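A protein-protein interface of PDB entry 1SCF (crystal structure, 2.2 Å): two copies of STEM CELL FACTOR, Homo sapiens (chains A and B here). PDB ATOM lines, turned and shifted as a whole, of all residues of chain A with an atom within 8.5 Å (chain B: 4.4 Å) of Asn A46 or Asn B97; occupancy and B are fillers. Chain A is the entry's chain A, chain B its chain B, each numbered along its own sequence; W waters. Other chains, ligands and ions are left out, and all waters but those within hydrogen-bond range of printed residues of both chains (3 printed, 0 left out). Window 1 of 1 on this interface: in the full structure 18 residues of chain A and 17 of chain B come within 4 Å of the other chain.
The backbone carbonyl oxygen (O) of Asn A46 sits at hydrogen-bond distance from the side-chain amide nitrogen (ND2) of Asn B97. OG of Ser A92 lies within hydrogen-bond range of ND2 of Asn B46, 2.8 Å away. N of Asn A97 lies within hydrogen-bond range of OD1 of Asn B46 (2.9 Å).
The side-chain amide nitrogen of Asn A46 lies within hydrogen-bond range of the side-chain amide oxygen of Asn A97, 3.3 Å away. The backbone carbonyl oxygen (O) of Asn B46 sits at hydrogen-bond distance from the side-chain amide nitrogen (ND2) of Asn B97 (3.4 Å). OG of Ser B96 lies within hydrogen-bond range of OG of Ser B99 (3.2 Å).
Ile B91 touches Lys A42. Ala A45 touches Phe B88. Phe B88 touches Asn A46 (CE1 to O, 3.4 Å). Ile B91 touches Asn A46. OD1 of Asn A46 touches CA of Ser B96, at 3.8 Å. C of Leu A47 touches CE1 of Phe B88 (3.5 Å). Leu B47 touches Phe A88. Asn B46 touches Leu A95. Ile B91 touches Leu A95. Ser A96 touches Asn B46.
Asn A46 touches four residues of chain B. Of the printed residues of chain B, Leu A95 touches Asn B46 and Ile B91. Pro A137 touches none of the printed residues of chain B. Printed residues of chain A within 4 Å of Asn B46: Phe A88 (3.5 Å), Ser A92 (2.8 Å), Leu A95 (3.6 Å), Ser A96 (3.4 Å) and Asn A97 (2.9 Å). Of the printed residues of chain A, Phe B88 touches Ala A45 (3.6 Å), Asn A46 (3.4 Å), Leu A47 (3.5 Å) and Pro A48 (3.5 Å). Of chain A, only Asn A46 (3.8 Å) comes within 4 Å of Ser B96. Asn B97 touches just one residue of chain A: Asn A46. Ile B101 touches none of the printed residues of chain A. The nearest residue of chain B that does not touch Asn A46 is Asn B46 (4.1 Å). The nearest printed residue of chain B that does not touch Ala A45 is Asn B97 (5.8 Å).
Hydrophobic or aromatic side chains of chain A that line the printed part of chain B: Ala A45, Pro A48, Phe A88 and Leu A95. Along chain A the printed residues that touch a printed residue of chain B span positions 42 to 97. Of the 11 printed residues of chain B, 6 touch a printed residue of chain A. Printed residues of chain B that touch a printed residue of chain A: Asn B46, Leu B47, Phe B88, Ile B91, Ser B96 and Asn B97. Hydrophobic or aromatic side chains of chain B that line the printed part of chain A: Phe B88 and Ile B91. Along chain B the printed residues that touch a printed residue of chain A span positions 46 to 97. Among the printed residues, 16 pairs touch across the chains. Among the printed residues, no Asp or Glu carboxylate lies within 4 Å of a Lys or Arg side-chain nitrogen of the other chain.
Asn A46 touches Phe B88, and with the chains exchanged Phe A88 touches Asn B46. Asn A46 touches Ser B96, and with the chains exchanged Ser A96 touches Asn B46. Asn A46 touches Asn B97, and with the chains exchanged Asn A97 touches Asn B46. Leu A47 touches Phe B88, and with the chains exchanged Phe A88 touches Leu B47. Positions printed for both chains: 43, 46, 47, 88, 96, 97, 98 and 100. Of the 16 pairs that touch across the chains among the printed residues, 8 have their exchanged pair printed and touching as well.
Water W3 lies within hydrogen-bond range of O of Asn B46 (2.7 Å), O of Asn A46 (2.9 Å) and ND2 of Asn B97 (3.5 Å). Water W2 lies within hydrogen-bond range of OD1 of Asn B46 (2.8 Å), N of Tyr A98 (3.1 Å) and N of Asn A97 (3.4 Å). Water W1 lies within hydrogen-bond range of the side-chain amide oxygen of Asn A46, the backbone carbonyl oxygen of Ala A45 and the backbone NH of Tyr B98.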
ATOM      1  N   ASP A  39       4.011  10.591  22.844  1.00  0.00           N
ATOM      2  CA  ASP A  39       3.247  11.431  21.978  1.00  0.00           C
ATOM      3  C   ASP A  39       3.295  12.849  22.477  1.00  0.00           C
ATOM      4  O   ASP A  39       3.350  13.744  21.646  1.00  0.00           O
ATOM      5  CB  ASP A  39       1.840  10.853  21.808  1.00  0.00           C
ATOM      6  CG  ASP A  39       1.642   9.898  20.597  1.00  0.00           C
ATOM      7  OD1 ASP A  39       2.519   9.719  19.733  1.00  0.00           O
ATOM      8  OD2 ASP A  39       0.560   9.314  20.495  1.00  0.00           O
ATOM      9  N   VAL A  40       3.360  13.067  23.799  1.00  0.00           N
ATOM     10  CA  VAL A  40       3.566  14.390  24.357  1.00  0.00           C
ATOM     11  C   VAL A  40       4.866  15.015  23.892  1.00  0.00           C
ATOM     12  O   VAL A  40       4.834  16.163  23.468  1.00  0.00           O
ATOM     13  CB  VAL A  40       3.508  14.445  25.897  1.00  0.00           C
ATOM     14  CG1 VAL A  40       3.842  15.838  26.430  1.00  0.00           C
ATOM     15  CG2 VAL A  40       2.125  14.037  26.377  1.00  0.00           C
ATOM     16  N   THR A  41       6.013  14.341  23.927  1.00  0.00           N
ATOM     17  CA  THR A  41       7.242  14.916  23.406  1.00  0.00           C
ATOM     18  C   THR A  41       7.144  15.143  21.908  1.00  0.00           C
ATOM     19  O   THR A  41       7.604  16.198  21.484  1.00  0.00           O
ATOM     20  CB  THR A  41       8.533  14.106  23.763  1.00  0.00           C
ATOM     21  OG1 THR A  41       8.430  12.868  23.082  1.00  0.00           O
ATOM     22  CG2 THR A  41       8.657  13.881  25.248  1.00  0.00           C
ATOM     23  N   LYS A  42       6.553  14.229  21.106  1.00  0.00           N
ATOM     24  CA  LYS A  42       6.331  14.448  19.678  1.00  0.00           C
ATOM     25  C   LYS A  42       5.501  15.672  19.388  1.00  0.00           C
ATOM     26  O   LYS A  42       5.795  16.398  18.444  1.00  0.00           O
ATOM     27  CB  LYS A  42       5.697  13.235  18.986  1.00  0.00           C
ATOM     28  CG  LYS A  42       6.688  12.086  18.959  1.00  0.00           C
ATOM     29  CD  LYS A  42       6.225  10.874  18.153  1.00  0.00           C
ATOM     30  CE  LYS A  42       7.375   9.840  17.951  1.00  0.00           C
ATOM     31  NZ  LYS A  42       7.607   8.940  19.081  1.00  0.00           N
ATOM     32  N   LEU A  43       4.491  15.951  20.219  1.00  0.00           N
ATOM     33  CA  LEU A  43       3.618  17.103  20.044  1.00  0.00           C
ATOM     34  C   LEU A  43       4.372  18.361  20.358  1.00  0.00           C
ATOM     35  O   LEU A  43       4.488  19.218  19.501  1.00  0.00           O
ATOM     36  CB  LEU A  43       2.400  17.006  20.953  1.00  0.00           C
ATOM     37  CG  LEU A  43       1.348  18.112  20.850  1.00  0.00           C
ATOM     38  CD1 LEU A  43       0.794  18.238  19.461  1.00  0.00           C
ATOM     39  CD2 LEU A  43       0.259  17.860  21.852  1.00  0.00           C
ATOM     40  N   VAL A  44       4.937  18.436  21.563  1.00  0.00           N
ATOM     41  CA  VAL A  44       5.876  19.489  21.919  1.00  0.00           C
ATOM     42  C   VAL A  44       6.958  19.727  20.889  1.00  0.00           C
ATOM     43  O   VAL A  44       7.205  20.873  20.554  1.00  0.00           O
ATOM     44  CB  VAL A  44       6.469  19.279  23.277  1.00  0.00           C
ATOM     45  CG1 VAL A  44       7.482  20.349  23.635  1.00  0.00           C
ATOM     46  CG2 VAL A  44       5.342  19.464  24.235  1.00  0.00           C
ATOM     47  N   ALA A  45       7.531  18.721  20.268  1.00  0.00           N
ATOM     48  CA  ALA A  45       8.462  18.973  19.198  1.00  0.00           C
ATOM     49  C   ALA A  45       7.760  19.457  17.949  1.00  0.00           C
ATOM     50  O   ALA A  45       8.360  20.105  17.099  1.00  0.00           O
ATOM     51  CB  ALA A  45       9.155  17.667  18.890  1.00  0.00           C
ATOM     52  N   ASN A  46       6.486  19.152  17.763  1.00  0.00           N
ATOM     53  CA  ASN A  46       5.810  19.564  16.550  1.00  0.00           C
ATOM     54  C   ASN A  46       4.956  20.819  16.754  1.00  0.00           C
ATOM     55  O   ASN A  46       4.183  21.199  15.881  1.00  0.00           O
ATOM     56  CB  ASN A  46       5.033  18.360  16.052  1.00  0.00           C
ATOM     57  CG  ASN A  46       5.026  18.312  14.547  1.00  0.00           C
ATOM     58  OD1 ASN A  46       6.059  18.503  13.925  1.00  0.00           O
ATOM     59  ND2 ASN A  46       3.883  18.105  13.880  1.00  0.00           N
ATOM     60  N   LEU A  47       5.099  21.495  17.892  1.00  0.00           N
ATOM     61  CA  LEU A  47       4.473  22.769  18.168  1.00  0.00           C
ATOM     62  C   LEU A  47       5.495  23.913  18.190  1.00  0.00           C
ATOM     63  O   LEU A  47       6.605  23.702  18.673  1.00  0.00           O
ATOM     64  CB  LEU A  47       3.708  22.722  19.510  1.00  0.00           C
ATOM     65  CG  LEU A  47       2.435  21.893  19.662  1.00  0.00           C
ATOM     66  CD1 LEU A  47       1.915  21.798  21.100  1.00  0.00           C
ATOM     67  CD2 LEU A  47       1.374  22.481  18.764  1.00  0.00           C
ATOM     68  N   PRO A  48       5.248  25.143  17.703  1.00  0.00           N
ATOM     69  CA  PRO A  48       6.243  26.213  17.702  1.00  0.00           C
ATOM     70  C   PRO A  48       6.600  26.596  19.128  1.00  0.00           C
ATOM     71  O   PRO A  48       5.696  26.739  19.941  1.00  0.00           O
ATOM     72  CB  PRO A  48       5.501  27.351  17.047  1.00  0.00           C
ATOM     73  CG  PRO A  48       4.307  26.731  16.340  1.00  0.00           C
ATOM     74  CD  PRO A  48       3.928  25.671  17.342  1.00  0.00           C
ATOM     75  N   LYS A  49       7.868  26.814  19.490  1.00  0.00           N
ATOM     76  CA  LYS A  49       8.281  27.156  20.873  1.00  0.00           C
ATOM     77  C   LYS A  49       7.665  28.406  21.519  1.00  0.00           C
ATOM     78  O   LYS A  49       7.609  28.577  22.746  1.00  0.00           O
ATOM     79  CB  LYS A  49       9.837  27.242  20.979  1.00  0.00           C
ATOM     80  CG  LYS A  49      10.544  25.931  20.581  1.00  0.00           C
ATOM     81  CD  LYS A  49      12.063  26.176  20.445  1.00  0.00           C
ATOM     82  CE  LYS A  49      12.884  25.155  19.655  1.00  0.00           C
ATOM     83  NZ  LYS A  49      14.165  25.769  19.302  1.00  0.00           N
ATOM     84  N   TYR A  51       4.425  29.579  20.488  1.00  0.00           N
ATOM     85  CA  TYR A  51       3.010  29.509  20.451  1.00  0.00           C
ATOM     86  C   TYR A  51       2.603  29.354  21.890  1.00  0.00           C
ATOM     87  O   TYR A  51       2.887  28.356  22.525  1.00  0.00           O
ATOM     88  CB  TYR A  51       2.614  28.313  19.637  1.00  0.00           C
ATOM     89  CG  TYR A  51       1.101  28.187  19.534  1.00  0.00           C
ATOM     90  CD1 TYR A  51       0.407  29.261  19.020  1.00  0.00           C
ATOM     91  CD2 TYR A  51       0.455  27.031  19.939  1.00  0.00           C
ATOM     92  CE1 TYR A  51      -0.941  29.194  18.890  1.00  0.00           C
ATOM     93  CE2 TYR A  51      -0.916  26.959  19.788  1.00  0.00           C
ATOM     94  CZ  TYR A  51      -1.594  28.045  19.254  1.00  0.00           C
ATOM     95  OH  TYR A  51      -2.965  28.004  19.033  1.00  0.00           O
ATOM     96  N   PHE A  88      -6.075  22.993  14.676  1.00  0.00           N
ATOM     97  CA  PHE A  88      -5.412  22.054  13.793  1.00  0.00           C
ATOM     98  C   PHE A  88      -6.405  21.361  12.887  1.00  0.00           C
ATOM     99  O   PHE A  88      -7.598  21.294  13.152  1.00  0.00           O
ATOM    100  CB  PHE A  88      -4.611  21.030  14.611  1.00  0.00           C
ATOM    101  CG  PHE A  88      -3.489  21.646  15.418  1.00  0.00           C
ATOM    102  CD1 PHE A  88      -2.295  21.948  14.812  1.00  0.00           C
ATOM    103  CD2 PHE A  88      -3.713  21.972  16.739  1.00  0.00           C
ATOM    104  CE1 PHE A  88      -1.354  22.622  15.529  1.00  0.00           C
ATOM    105  CE2 PHE A  88      -2.774  22.686  17.447  1.00  0.00           C
ATOM    106  CZ  PHE A  88      -1.604  23.010  16.818  1.00  0.00           C
ATOM    107  N   SER A  92      -4.894  14.952   7.602  1.00  0.00           N
ATOM    108  CA  SER A  92      -3.445  14.913   7.688  1.00  0.00           C
ATOM    109  C   SER A  92      -3.041  13.443   7.632  1.00  0.00           C
ATOM    110  O   SER A  92      -3.558  12.598   8.372  1.00  0.00           O
ATOM    111  CB  SER A  92      -3.019  15.569   9.033  1.00  0.00           C
ATOM    112  OG  SER A  92      -1.703  16.106   9.053  1.00  0.00           O
ATOM    113  N   GLY A  94      -0.179  10.489   8.302  1.00  0.00           N
ATOM    114  CA  GLY A  94       0.853  10.301   9.296  1.00  0.00           C
ATOM    115  C   GLY A  94       0.577  11.061  10.568  1.00  0.00           C
ATOM    116  O   GLY A  94      -0.517  11.056  11.129  1.00  0.00           O
ATOM    117  N   LEU A  95       1.651  11.742  10.949  1.00  0.00           N
ATOM    118  CA  LEU A  95       1.701  12.557  12.164  1.00  0.00           C
ATOM    119  C   LEU A  95       0.683  13.679  12.094  1.00  0.00           C
ATOM    120  O   LEU A  95       0.705  14.488  11.166  1.00  0.00           O
ATOM    121  CB  LEU A  95       3.137  13.176  12.355  1.00  0.00           C
ATOM    122  CG  LEU A  95       3.547  13.936  13.668  1.00  0.00           C
ATOM    123  CD1 LEU A  95       3.218  13.177  14.969  1.00  0.00           C
ATOM    124  CD2 LEU A  95       5.037  14.292  13.605  1.00  0.00           C
ATOM    125  N   SER A  96      -0.184  13.718  13.100  1.00  0.00           N
ATOM    126  CA  SER A  96      -1.220  14.716  13.192  1.00  0.00           C
ATOM    127  C   SER A  96      -1.222  15.272  14.598  1.00  0.00           C
ATOM    128  O   SER A  96      -1.347  14.536  15.558  1.00  0.00           O
ATOM    129  CB  SER A  96      -2.526  14.020  12.828  1.00  0.00           C
ATOM    130  OG  SER A  96      -3.671  14.815  13.022  1.00  0.00           O
ATOM    131  N   ASN A  97      -1.057  16.559  14.793  1.00  0.00           N
ATOM    132  CA  ASN A  97      -1.280  17.169  16.088  1.00  0.00           C
ATOM    133  C   ASN A  97      -2.684  17.088  16.548  1.00  0.00           C
ATOM    134  O   ASN A  97      -2.886  16.909  17.736  1.00  0.00           O
ATOM    135  CB  ASN A  97      -0.933  18.624  16.071  1.00  0.00           C
ATOM    136  CG  ASN A  97       0.556  18.804  15.898  1.00  0.00           C
ATOM    137  OD1 ASN A  97       1.352  17.862  16.013  1.00  0.00           O
ATOM    138  ND2 ASN A  97       0.951  20.039  15.612  1.00  0.00           N
ATOM    139  N   TYR A  98      -3.651  17.247  15.641  1.00  0.00           N
ATOM    140  CA  TYR A  98      -5.044  16.927  15.954  1.00  0.00           C
ATOM    141  C   TYR A  98      -5.184  15.539  16.559  1.00  0.00           C
ATOM    142  O   TYR A  98      -5.751  15.462  17.647  1.00  0.00           O
ATOM    143  CB  TYR A  98      -6.010  16.978  14.717  1.00  0.00           C
ATOM    144  CG  TYR A  98      -7.479  17.125  15.089  1.00  0.00           C
ATOM    145  CD1 TYR A  98      -8.010  18.384  15.216  1.00  0.00           C
ATOM    146  CD2 TYR A  98      -8.285  16.012  15.296  1.00  0.00           C
ATOM    147  CE1 TYR A  98      -9.333  18.544  15.550  1.00  0.00           C
ATOM    148  CE2 TYR A  98      -9.608  16.151  15.654  1.00  0.00           C
ATOM    149  CZ  TYR A  98     -10.104  17.423  15.765  1.00  0.00           C
ATOM    150  OH  TYR A  98     -11.422  17.614  16.100  1.00  0.00           O
ATOM    151  N   ILE A 100      -2.964  13.580  18.079  1.00  0.00           N
ATOM    152  CA  ILE A 100      -2.247  13.520  19.353  1.00  0.00           C
ATOM    153  C   ILE A 100      -3.056  14.197  20.433  1.00  0.00           C
ATOM    154  O   ILE A 100      -3.450  13.556  21.388  1.00  0.00           O
ATOM    155  CB  ILE A 100      -0.762  14.055  19.244  1.00  0.00           C
ATOM    156  CG1 ILE A 100       0.062  13.227  18.216  1.00  0.00           C
ATOM    157  CG2 ILE A 100      -0.072  13.965  20.606  1.00  0.00           C
ATOM    158  CD1 ILE A 100       1.521  13.668  18.012  1.00  0.00           C
ATOM    159  N   PRO A 137       4.380  25.636  24.790  1.00  0.00           N
ATOM    160  CA  PRO A 137       4.040  24.207  24.668  1.00  0.00           C
ATOM    161  C   PRO A 137       4.742  23.310  25.697  1.00  0.00           C
ATOM    162  O   PRO A 137       4.114  22.583  26.446  1.00  0.00           O
ATOM    163  CB  PRO A 137       4.481  23.955  23.257  1.00  0.00           C
ATOM    164  CG  PRO A 137       4.170  25.270  22.578  1.00  0.00           C
ATOM    165  CD  PRO A 137       4.711  26.266  23.527  1.00  0.00           C
ATOM    166  N   LEU B  43       2.180  20.452   6.424  1.00  0.00           N
ATOM    167  CA  LEU B  43       2.731  21.474   7.279  1.00  0.00           C
ATOM    168  C   LEU B  43       1.651  22.445   7.666  1.00  0.00           C
ATOM    169  O   LEU B  43       1.548  22.662   8.861  1.00  0.00           O
ATOM    170  CB  LEU B  43       3.892  22.207   6.607  1.00  0.00           C
ATOM    171  CG  LEU B  43       4.522  23.357   7.321  1.00  0.00           C
ATOM    172  CD1 LEU B  43       5.068  22.912   8.633  1.00  0.00           C
ATOM    173  CD2 LEU B  43       5.636  23.897   6.515  1.00  0.00           C
ATOM    174  N   ASN B  46      -0.673  20.947  10.186  1.00  0.00           N
ATOM    175  CA  ASN B  46      -0.125  20.802  11.504  1.00  0.00           C
ATOM    176  C   ASN B  46       0.417  22.074  12.089  1.00  0.00           C
ATOM    177  O   ASN B  46       1.071  21.992  13.101  1.00  0.00           O
ATOM    178  CB  ASN B  46       0.907  19.739  11.496  1.00  0.00           C
ATOM    179  CG  ASN B  46       0.195  18.408  11.391  1.00  0.00           C
ATOM    180  OD1 ASN B  46      -0.349  17.870  12.358  1.00  0.00           O
ATOM    181  ND2 ASN B  46       0.162  17.870  10.177  1.00  0.00           N
ATOM    182  N   LEU B  47       0.173  23.258  11.550  1.00  0.00           N
ATOM    183  CA  LEU B  47       0.530  24.509  12.200  1.00  0.00           C
ATOM    184  C   LEU B  47      -0.708  25.069  12.866  1.00  0.00           C
ATOM    185  O   LEU B  47      -1.770  24.950  12.261  1.00  0.00           O
ATOM    186  CB  LEU B  47       1.090  25.520  11.172  1.00  0.00           C
ATOM    187  CG  LEU B  47       2.520  25.313  10.621  1.00  0.00           C
ATOM    188  CD1 LEU B  47       2.857  26.285   9.497  1.00  0.00           C
ATOM    189  CD2 LEU B  47       3.523  25.431  11.761  1.00  0.00           C
ATOM    190  N   PHE B  88      10.879  24.673  15.857  1.00  0.00           N
ATOM    191  CA  PHE B  88      10.603  23.248  15.975  1.00  0.00           C
ATOM    192  C   PHE B  88      11.875  22.495  16.316  1.00  0.00           C
ATOM    193  O   PHE B  88      12.961  23.040  16.146  1.00  0.00           O
ATOM    194  CB  PHE B  88       9.996  22.656  14.697  1.00  0.00           C
ATOM    195  CG  PHE B  88       8.677  23.321  14.389  1.00  0.00           C
ATOM    196  CD1 PHE B  88       7.538  22.855  14.973  1.00  0.00           C
ATOM    197  CD2 PHE B  88       8.653  24.460  13.589  1.00  0.00           C
ATOM    198  CE1 PHE B  88       6.376  23.564  14.786  1.00  0.00           C
ATOM    199  CE2 PHE B  88       7.491  25.183  13.436  1.00  0.00           C
ATOM    200  CZ  PHE B  88       6.351  24.721  14.041  1.00  0.00           C
ATOM    201  N   ILE B  91      11.802  15.172  15.005  1.00  0.00           N
ATOM    202  CA  ILE B  91      11.067  13.949  15.342  1.00  0.00           C
ATOM    203  C   ILE B  91      11.400  12.895  14.283  1.00  0.00           C
ATOM    204  O   ILE B  91      11.143  13.079  13.083  1.00  0.00           O
ATOM    205  CB  ILE B  91       9.531  14.193  15.290  1.00  0.00           C
ATOM    206  CG1 ILE B  91       9.062  15.338  16.181  1.00  0.00           C
ATOM    207  CG2 ILE B  91       8.787  12.934  15.685  1.00  0.00           C
ATOM    208  CD1 ILE B  91       7.601  15.740  15.931  1.00  0.00           C
ATOM    209  N   SER B  96       7.863  15.535  10.008  1.00  0.00           N
ATOM    210  CA  SER B  96       7.578  16.454  11.055  1.00  0.00           C
ATOM    211  C   SER B  96       7.670  17.867  10.476  1.00  0.00           C
ATOM    212  O   SER B  96       8.204  18.063   9.379  1.00  0.00           O
ATOM    213  CB  SER B  96       8.534  16.150  12.168  1.00  0.00           C
ATOM    214  OG  SER B  96       9.881  16.209  11.764  1.00  0.00           O
ATOM    215  N   ASN B  97       7.118  18.887  11.159  1.00  0.00           N
ATOM    216  CA  ASN B  97       7.187  20.283  10.708  1.00  0.00           C
ATOM    217  C   ASN B  97       8.632  20.694  10.517  1.00  0.00           C
ATOM    218  O   ASN B  97       8.930  21.397   9.566  1.00  0.00           O
ATOM    219  CB  ASN B  97       6.491  21.240  11.705  1.00  0.00           C
ATOM    220  CG  ASN B  97       4.981  21.072  11.890  1.00  0.00           C
ATOM    221  OD1 ASN B  97       4.263  20.638  10.998  1.00  0.00           O
ATOM    222  ND2 ASN B  97       4.429  21.379  13.060  1.00  0.00           N
ATOM    223  N   TYR B  98       9.516  20.189  11.397  1.00  0.00           N
ATOM    224  CA  TYR B  98      10.958  20.370  11.286  1.00  0.00           C
ATOM    225  C   TYR B  98      11.440  19.845   9.960  1.00  0.00           C
ATOM    226  O   TYR B  98      11.937  20.626   9.170  1.00  0.00           O
ATOM    227  CB  TYR B  98      11.797  19.696  12.406  1.00  0.00           C
ATOM    228  CG  TYR B  98      13.270  20.135  12.473  1.00  0.00           C
ATOM    229  CD1 TYR B  98      14.230  19.663  11.574  1.00  0.00           C
ATOM    230  CD2 TYR B  98      13.628  21.078  13.419  1.00  0.00           C
ATOM    231  CE1 TYR B  98      15.499  20.210  11.577  1.00  0.00           C
ATOM    232  CE2 TYR B  98      14.905  21.612  13.446  1.00  0.00           C
ATOM    233  CZ  TYR B  98      15.817  21.189  12.506  1.00  0.00           C
ATOM    234  OH  TYR B  98      17.074  21.778  12.504  1.00  0.00           O
ATOM    235  N   SER B  99      11.298  18.573   9.657  1.00  0.00           N
ATOM    236  CA  SER B  99      11.704  18.077   8.360  1.00  0.00           C
ATOM    237  C   SER B  99      11.079  18.787   7.196  1.00  0.00           C
ATOM    238  O   SER B  99      11.705  18.998   6.171  1.00  0.00           O
ATOM    239  CB  SER B  99      11.331  16.647   8.236  1.00  0.00           C
ATOM    240  OG  SER B  99      11.964  16.048   9.345  1.00  0.00           O
ATOM    241  N   ILE B 100       9.825  19.192   7.306  1.00  0.00           N
ATOM    242  CA  ILE B 100       9.190  19.789   6.147  1.00  0.00           C
ATOM    243  C   ILE B 100       9.758  21.166   5.909  1.00  0.00           C
ATOM    244  O   ILE B 100      10.140  21.427   4.786  1.00  0.00           O
ATOM    245  CB  ILE B 100       7.683  19.808   6.322  1.00  0.00           C
ATOM    246  CG1 ILE B 100       7.136  18.402   6.282  1.00  0.00           C
ATOM    247  CG2 ILE B 100       7.045  20.585   5.190  1.00  0.00           C
ATOM    248  CD1 ILE B 100       5.629  18.350   6.636  1.00  0.00           C
ATOM    249  N   ILE B 101       9.826  21.989   6.960  1.00  0.00           N
ATOM    250  CA  ILE B 101      10.275  23.366   6.859  1.00  0.00           C
ATOM    251  C   ILE B 101      11.710  23.331   6.394  1.00  0.00           C
ATOM    252  O   ILE B 101      12.000  24.028   5.441  1.00  0.00           O
ATOM    253  CB  ILE B 101      10.169  24.182   8.167  1.00  0.00           C
ATOM    254  CG1 ILE B 101       8.755  24.272   8.676  1.00  0.00           C
ATOM    255  CG2 ILE B 101      10.640  25.610   7.936  1.00  0.00           C
ATOM    256  CD1 ILE B 101       8.672  24.610  10.157  1.00  0.00           C
HETATM  257  O   HOH W   1       8.860  19.156  14.233  1.00  0.00           O
HETATM  258  O   HOH W   2      -3.114  18.359  12.842  1.00  0.00           O
HETATM  259  O   HOH W   3       2.326  23.247  15.101  1.00  0.00           O
